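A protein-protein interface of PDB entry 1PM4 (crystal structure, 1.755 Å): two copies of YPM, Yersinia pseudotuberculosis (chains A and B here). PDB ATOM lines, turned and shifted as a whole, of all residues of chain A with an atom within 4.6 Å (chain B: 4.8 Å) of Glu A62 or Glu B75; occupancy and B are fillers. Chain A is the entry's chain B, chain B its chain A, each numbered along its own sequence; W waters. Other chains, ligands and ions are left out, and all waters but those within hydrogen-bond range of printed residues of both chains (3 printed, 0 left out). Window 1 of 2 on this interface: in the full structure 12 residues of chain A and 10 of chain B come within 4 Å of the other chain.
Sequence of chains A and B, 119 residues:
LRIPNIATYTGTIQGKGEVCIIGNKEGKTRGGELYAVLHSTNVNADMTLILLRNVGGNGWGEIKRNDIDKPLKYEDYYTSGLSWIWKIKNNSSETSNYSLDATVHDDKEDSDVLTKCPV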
ATOM      1  N   ILE A  50     -14.651 -14.379  -5.762  1.00  0.00           N
ATOM      2  CA  ILE A  50     -15.028 -15.795  -5.968  1.00  0.00           C
ATOM      3  C   ILE A  50     -16.317 -15.938  -6.775  1.00  0.00           C
ATOM      4  O   ILE A  50     -17.314 -15.329  -6.468  1.00  0.00           O
ATOM      5  CB  ILE A  50     -15.119 -16.642  -4.624  1.00  0.00           C
ATOM      6  CG1 ILE A  50     -13.909 -16.474  -3.761  1.00  0.00           C
ATOM      7  CG2 ILE A  50     -15.465 -18.082  -4.884  1.00  0.00           C
ATOM      8  CD1 ILE A  50     -14.101 -16.876  -2.283  1.00  0.00           C
ATOM      9  N   LEU A  51     -16.287 -16.740  -7.851  1.00  0.00           N
ATOM     10  CA  LEU A  51     -17.471 -17.049  -8.606  1.00  0.00           C
ATOM     11  C   LEU A  51     -18.070 -18.329  -8.089  1.00  0.00           C
ATOM     12  O   LEU A  51     -17.389 -19.377  -8.077  1.00  0.00           O
ATOM     13  CB  LEU A  51     -17.132 -17.206 -10.106  1.00  0.00           C
ATOM     14  CG  LEU A  51     -18.335 -17.687 -10.939  1.00  0.00           C
ATOM     15  CD1 LEU A  51     -19.527 -16.755 -10.950  1.00  0.00           C
ATOM     16  CD2 LEU A  51     -17.909 -17.921 -12.382  1.00  0.00           C
ATOM     17  N   LEU A  52     -19.310 -18.274  -7.654  1.00  0.00           N
ATOM     18  CA  LEU A  52     -20.046 -19.442  -7.225  1.00  0.00           C
ATOM     19  C   LEU A  52     -21.193 -19.699  -8.215  1.00  0.00           C
ATOM     20  O   LEU A  52     -21.827 -18.776  -8.737  1.00  0.00           O
ATOM     21  CB  LEU A  52     -20.662 -19.236  -5.835  1.00  0.00           C
ATOM     22  CG  LEU A  52     -19.713 -18.719  -4.766  1.00  0.00           C
ATOM     23  CD1 LEU A  52     -20.461 -18.191  -3.556  1.00  0.00           C
ATOM     24  CD2 LEU A  52     -18.844 -19.799  -4.402  1.00  0.00           C
ATOM     25  N   GLY A  61     -21.481 -23.879  -5.152  1.00  0.00           N
ATOM     26  CA  GLY A  61     -20.067 -24.261  -5.153  1.00  0.00           C
ATOM     27  C   GLY A  61     -19.169 -23.323  -5.929  1.00  0.00           C
ATOM     28  O   GLY A  61     -19.592 -22.737  -6.916  1.00  0.00           O
ATOM     29  N   GLU A  62     -17.928 -23.176  -5.490  1.00  0.00           N
ATOM     30  CA  GLU A  62     -16.975 -22.298  -6.200  1.00  0.00           C
ATOM     31  C   GLU A  62     -16.627 -22.829  -7.561  1.00  0.00           C
ATOM     32  O   GLU A  62     -16.331 -24.025  -7.699  1.00  0.00           O
ATOM     33  CB  GLU A  62     -15.729 -22.040  -5.344  1.00  0.00           C
ATOM     34  CG  GLU A  62     -14.490 -21.529  -6.064  1.00  0.00           C
ATOM     35  CD  GLU A  62     -13.370 -21.174  -5.126  1.00  0.00           C
ATOM     36  OE1 GLU A  62     -13.506 -21.227  -3.895  1.00  0.00           O
ATOM     37  OE2 GLU A  62     -12.283 -20.778  -5.608  1.00  0.00           O
ATOM     38  N   ILE A  63     -16.606 -21.941  -8.554  1.00  0.00           N
ATOM     39  CA  ILE A  63     -16.002 -22.265  -9.871  1.00  0.00           C
ATOM     40  C   ILE A  63     -14.531 -21.889  -9.960  1.00  0.00           C
ATOM     41  O   ILE A  63     -13.678 -22.713 -10.301  1.00  0.00           O
ATOM     42  CB  ILE A  63     -16.762 -21.557 -10.971  1.00  0.00           C
ATOM     43  CG1 ILE A  63     -18.232 -21.961 -10.958  1.00  0.00           C
ATOM     44  CG2 ILE A  63     -16.138 -21.856 -12.348  1.00  0.00           C
ATOM     45  CD1 ILE A  63     -18.534 -23.487 -11.102  1.00  0.00           C
ATOM     46  N   LYS A  64     -14.248 -20.656  -9.605  1.00  0.00           N
ATOM     47  CA  LYS A  64     -12.906 -20.141  -9.623  1.00  0.00           C
ATOM     48  C   LYS A  64     -12.893 -18.831  -8.851  1.00  0.00           C
ATOM     49  O   LYS A  64     -13.932 -18.299  -8.444  1.00  0.00           O
ATOM     50  CB  LYS A  64     -12.385 -19.981 -11.069  1.00  0.00           C
ATOM     51  CG  LYS A  64     -12.994 -18.853 -11.866  1.00  0.00           C
ATOM     52  CD  LYS A  64     -12.222 -18.576 -13.194  1.00  0.00           C
ATOM     53  CE  LYS A  64     -12.512 -19.580 -14.242  1.00  0.00           C
ATOM     54  NZ  LYS A  64     -11.670 -19.302 -15.473  1.00  0.00           N
ATOM     55  N   ARG A  65     -11.674 -18.357  -8.645  1.00  0.00           N
ATOM     56  CA  ARG A  65     -11.427 -17.132  -7.892  1.00  0.00           C
ATOM     57  C   ARG A  65     -10.242 -16.381  -8.435  1.00  0.00           C
ATOM     58  O   ARG A  65      -9.354 -16.993  -9.089  1.00  0.00           O
ATOM     59  CB  ARG A  65     -11.168 -17.402  -6.420  1.00  0.00           C
ATOM     60  CG  ARG A  65      -9.917 -18.173  -6.061  1.00  0.00           C
ATOM     61  CD  ARG A  65      -9.678 -18.252  -4.597  1.00  0.00           C
ATOM     62  NE  ARG A  65     -10.683 -19.088  -3.945  1.00  0.00           N
ATOM     63  CZ  ARG A  65     -10.966 -19.049  -2.635  1.00  0.00           C
ATOM     64  NH1 ARG A  65     -10.268 -18.289  -1.813  1.00  0.00           N
ATOM     65  NH2 ARG A  65     -11.897 -19.838  -2.114  1.00  0.00           N
ATOM     66  N   LYS A  87     -18.760 -13.429  -4.994  1.00  0.00           N
ATOM     67  CA  LYS A  87     -18.439 -13.198  -3.580  1.00  0.00           C
ATOM     68  C   LYS A  87     -17.159 -12.348  -3.518  1.00  0.00           C
ATOM     69  O   LYS A  87     -16.124 -12.784  -4.015  1.00  0.00           O
ATOM     70  CB  LYS A  87     -18.224 -14.515  -2.811  1.00  0.00           C
ATOM     71  CG  LYS A  87     -17.859 -14.393  -1.378  1.00  0.00           C
ATOM     72  CD  LYS A  87     -17.977 -15.734  -0.653  1.00  0.00           C
ATOM     73  CE  LYS A  87     -17.656 -15.591   0.783  1.00  0.00           C
ATOM     74  NZ  LYS A  87     -17.877 -16.958   1.423  1.00  0.00           N
ATOM     75  N   LYS A  89     -14.502 -10.890  -0.951  1.00  0.00           N
ATOM     76  CA  LYS A  89     -13.891 -10.985   0.365  1.00  0.00           C
ATOM     77  C   LYS A  89     -12.798  -9.944   0.566  1.00  0.00           C
ATOM     78  O   LYS A  89     -11.891  -9.837  -0.243  1.00  0.00           O
ATOM     79  CB  LYS A  89     -13.245 -12.356   0.553  1.00  0.00           C
ATOM     80  CG  LYS A  89     -14.200 -13.488   0.619  1.00  0.00           C
ATOM     81  CD  LYS A  89     -13.507 -14.800   0.897  1.00  0.00           C
ATOM     82  CE  LYS A  89     -12.738 -14.864   2.227  1.00  0.00           C
ATOM     83  NZ  LYS A  89     -11.970 -16.209   2.206  1.00  0.00           N
ATOM     84  N   GLY B  32     -18.324 -24.820   3.550  1.00  0.00           N
ATOM     85  CA  GLY B  32     -17.339 -23.804   3.875  1.00  0.00           C
ATOM     86  C   GLY B  32     -16.079 -24.007   3.068  1.00  0.00           C
ATOM     87  O   GLY B  32     -16.146 -24.553   1.966  1.00  0.00           O
ATOM     88  N   GLU B  33     -14.949 -23.557   3.583  1.00  0.00           N
ATOM     89  CA  GLU B  33     -13.743 -23.556   2.805  1.00  0.00           C
ATOM     90  C   GLU B  33     -12.925 -24.838   3.107  1.00  0.00           C
ATOM     91  O   GLU B  33     -12.761 -25.275   4.244  1.00  0.00           O
ATOM     92  CB  GLU B  33     -12.901 -22.290   3.077  1.00  0.00           C
ATOM     93  CG  GLU B  33     -11.455 -22.252   2.515  1.00  0.00           C
ATOM     94  CD  GLU B  33     -10.602 -21.103   3.100  1.00  0.00           C
ATOM     95  OE1 GLU B  33     -10.915 -19.934   2.793  1.00  0.00           O
ATOM     96  OE2 GLU B  33      -9.628 -21.345   3.871  1.00  0.00           O
ATOM     97  N   LYS B  64      -8.821 -27.968  -8.762  1.00  0.00           N
ATOM     98  CA  LYS B  64      -7.746 -27.045  -9.019  1.00  0.00           C
ATOM     99  C   LYS B  64      -6.465 -27.658  -8.479  1.00  0.00           C
ATOM    100  O   LYS B  64      -6.529 -28.661  -7.827  1.00  0.00           O
ATOM    101  CB  LYS B  64      -7.919 -25.695  -8.310  1.00  0.00           C
ATOM    102  CG  LYS B  64      -8.122 -25.807  -6.852  1.00  0.00           C
ATOM    103  CD  LYS B  64      -8.189 -24.362  -6.213  1.00  0.00           C
ATOM    104  CE  LYS B  64      -9.537 -23.742  -6.072  1.00  0.00           C
ATOM    105  NZ  LYS B  64      -9.226 -22.189  -5.811  1.00  0.00           N
ATOM    106  N   LYS B  73      -7.379 -23.053  -1.823  1.00  0.00           N
ATOM    107  CA  LYS B  73      -8.642 -22.802  -1.109  1.00  0.00           C
ATOM    108  C   LYS B  73      -9.783 -23.005  -2.055  1.00  0.00           C
ATOM    109  O   LYS B  73      -9.672 -22.622  -3.234  1.00  0.00           O
ATOM    110  CB  LYS B  73      -8.700 -21.371  -0.614  1.00  0.00           C
ATOM    111  CG  LYS B  73      -7.593 -20.982   0.291  1.00  0.00           C
ATOM    112  CD  LYS B  73      -7.903 -19.710   1.026  1.00  0.00           C
ATOM    113  CE  LYS B  73      -6.676 -19.170   1.706  1.00  0.00           C
ATOM    114  NZ  LYS B  73      -6.916 -17.907   2.369  1.00  0.00           N
ATOM    115  N   TYR B  74     -10.875 -23.567  -1.533  1.00  0.00           N
ATOM    116  CA  TYR B  74     -12.066 -23.874  -2.332  1.00  0.00           C
ATOM    117  C   TYR B  74     -13.322 -23.919  -1.462  1.00  0.00           C
ATOM    118  O   TYR B  74     -13.364 -24.605  -0.479  1.00  0.00           O
ATOM    119  CB  TYR B  74     -11.878 -25.222  -3.041  1.00  0.00           C
ATOM    120  CG  TYR B  74     -13.120 -25.769  -3.697  1.00  0.00           C
ATOM    121  CD1 TYR B  74     -13.510 -25.368  -4.940  1.00  0.00           C
ATOM    122  CD2 TYR B  74     -13.897 -26.662  -3.012  1.00  0.00           C
ATOM    123  CE1 TYR B  74     -14.697 -25.867  -5.483  1.00  0.00           C
ATOM    124  CE2 TYR B  74     -15.054 -27.166  -3.542  1.00  0.00           C
ATOM    125  CZ  TYR B  74     -15.450 -26.764  -4.751  1.00  0.00           C
ATOM    126  OH  TYR B  74     -16.626 -27.365  -5.220  1.00  0.00           O
ATOM    127  N   GLU B  75     -14.370 -23.195  -1.843  1.00  0.00           N
ATOM    128  CA  GLU B  75     -15.574 -23.129  -1.060  1.00  0.00           C
ATOM    129  C   GLU B  75     -16.614 -23.963  -1.684  1.00  0.00           C
ATOM    130  O   GLU B  75     -16.887 -23.788  -2.844  1.00  0.00           O
ATOM    131  CB  GLU B  75     -16.178 -21.689  -1.014  1.00  0.00           C
ATOM    132  CG  GLU B  75     -15.276 -20.637  -0.528  1.00  0.00           C
ATOM    133  CD  GLU B  75     -15.958 -19.374  -0.073  1.00  0.00           C
ATOM    134  OE1 GLU B  75     -17.149 -19.225  -0.200  1.00  0.00           O
ATOM    135  OE2 GLU B  75     -15.203 -18.574   0.353  1.00  0.00           O
ATOM    136  N   ASP B  76     -17.255 -24.786  -0.862  1.00  0.00           N
ATOM    137  CA  ASP B  76     -18.318 -25.695  -1.212  1.00  0.00           C
ATOM    138  C   ASP B  76     -19.451 -25.505  -0.211  1.00  0.00           C
ATOM    139  O   ASP B  76     -19.188 -25.536   0.988  1.00  0.00           O
ATOM    140  CB  ASP B  76     -17.749 -27.124  -1.017  1.00  0.00           C
ATOM    141  CG  ASP B  76     -18.584 -28.146  -1.631  1.00  0.00           C
ATOM    142  OD1 ASP B  76     -19.676 -28.383  -1.084  1.00  0.00           O
ATOM    143  OD2 ASP B  76     -18.237 -28.736  -2.682  1.00  0.00           O
ATOM    144  N   TYR B  77     -20.694 -25.348  -0.684  1.00  0.00           N
ATOM    145  CA  TYR B  77     -21.866 -25.221   0.206  1.00  0.00           C
ATOM    146  C   TYR B  77     -22.945 -26.223  -0.176  1.00  0.00           C
ATOM    147  O   TYR B  77     -24.153 -25.997   0.024  1.00  0.00           O
ATOM    148  CB  TYR B  77     -22.432 -23.806   0.144  1.00  0.00           C
ATOM    149  CG  TYR B  77     -21.390 -22.839   0.573  1.00  0.00           C
ATOM    150  CD1 TYR B  77     -21.060 -22.748   1.891  1.00  0.00           C
ATOM    151  CD2 TYR B  77     -20.643 -22.125  -0.351  1.00  0.00           C
ATOM    152  CE1 TYR B  77     -20.063 -21.936   2.326  1.00  0.00           C
ATOM    153  CE2 TYR B  77     -19.658 -21.287   0.068  1.00  0.00           C
ATOM    154  CZ  TYR B  77     -19.373 -21.193   1.412  1.00  0.00           C
ATOM    155  OH  TYR B  77     -18.373 -20.398   1.895  1.00  0.00           O
HETATM  156  O   HOH W   1      -9.317 -17.744   3.177  1.00  0.00           O
HETATM  157  O   HOH W   2     -20.321 -18.019   0.361  1.00  0.00           O
HETATM  158  O   HOH W   3     -10.988 -21.734  -7.502  1.00  0.00           O
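The side-chain carboxylate (OE1) of Glu B33 lies within salt-bridge range of the side-chain amino group (NZ) of Lys A89 (3.9 Å).
N of Glu A62 is in hydrogen-bond range of O of Glu B75 (2.9 Å).
The side-chain carboxylate of Glu B75 is in salt-bridge range of the side-chain amino group of Lys A87 (2.9 Å).
The side-chain carboxylate of Glu A62 is in salt-bridge range of the side-chain amino group of Lys B64 (3.4 Å).
The side-chain carboxylate (OE1) of Glu A62 is in salt-bridge range of the guanidinium group (NH2) of Arg A65 (2.8 Å).
The side-chain amino group (NZ) of Lys B64 sits at hydrogen-bond distance from the backbone carbonyl oxygen (O) of Lys B73, 2.7 Å away.
The side-chain carboxylate (OE1) of Glu B75 sits at hydrogen-bond distance from the side-chain hydroxyl (OH) of Tyr B77.
OH of Tyr B74 lies within hydrogen-bond range of OD2 of Asp B76, 3.3 Å away.
The backbone NH (N) of Ile A50 is in hydrogen-bond range of the backbone carbonyl oxygen (O) of Lys A87 (2.8 Å).
OE2 of Glu B75 touches CD1 of Ile A50 (3.3 Å).
Glu B75 touches Gly A61.
Lys B73 touches Glu A62 (O to OE2, 3.98 Å).
CE1 of Tyr B74 touches O of Glu A62, 3.3 Å away.
Arg A65 touches Lys B64.
Lys B73 touches Arg A65 (CB to NH1, 3.7 Å).
N of Tyr B74 touches NH2 of Arg A65, at 3.9 Å.
Arg A65 touches Glu B75.
Lys A87 touches Tyr B77.
Glu B75 touches just these residues of chain A: Ile A50 (3.3 Å), Gly A61 (3.9 Å), Glu A62 (2.9 Å), Arg A65 (3.8 Å) and Lys A87 (2.9 Å).
Of the printed residues of chain B, Lys A89 touches Glu B33 (3.9 Å).
Of the printed residues of chain A, Glu B33 touches Lys A89 (3.9 Å).
Of the printed residues of chain A, Lys B73 touches Glu A62 (3.98 Å) and Arg A65 (3.7 Å).
Asp B76 touches none of the printed residues of chain A.
Gly B32 touches none of the printed residues of chain A.
The nearest printed residue of chain A that does not touch Glu B33 is Arg A65 (4.9 Å).
Of the 10 printed residues of chain A, 6 touch a printed residue of chain B.
Of the 8 printed residues of chain B, 6 touch a printed residue of chain A.
Hydrophobic or aromatic side chains of chain B within 4 Å of the printed part of chain A: Tyr B74 and Tyr B77.
Among the printed residues, Asp or Glu carboxylates within 4 Å of a Lys or Arg side-chain nitrogen of the other chain: Glu A62 with Lys B64 (3.4 Å), Lys A87 with Glu B75 (2.9 Å) and Lys A89 with Glu B33 (3.9 Å).
Position printed for both chains: 64.
Water W3 lies within hydrogen-bond range of NZ of Lys B64 (2.5 Å) and OE2 of Glu A62 (2.5 Å).
Water W1 lies within hydrogen-bond range of the side-chain amino group of Lys B73 (2.5 Å), the side-chain carboxylate of Glu B33 (2.7 Å) and the side-chain amino group of Lys A89 (3.2 Å).
Water W2 lies within hydrogen-bond range of the side-chain amino group of Lys A87, the side-chain hydroxyl of Tyr B77 and the side-chain carboxylate of Glu B75.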
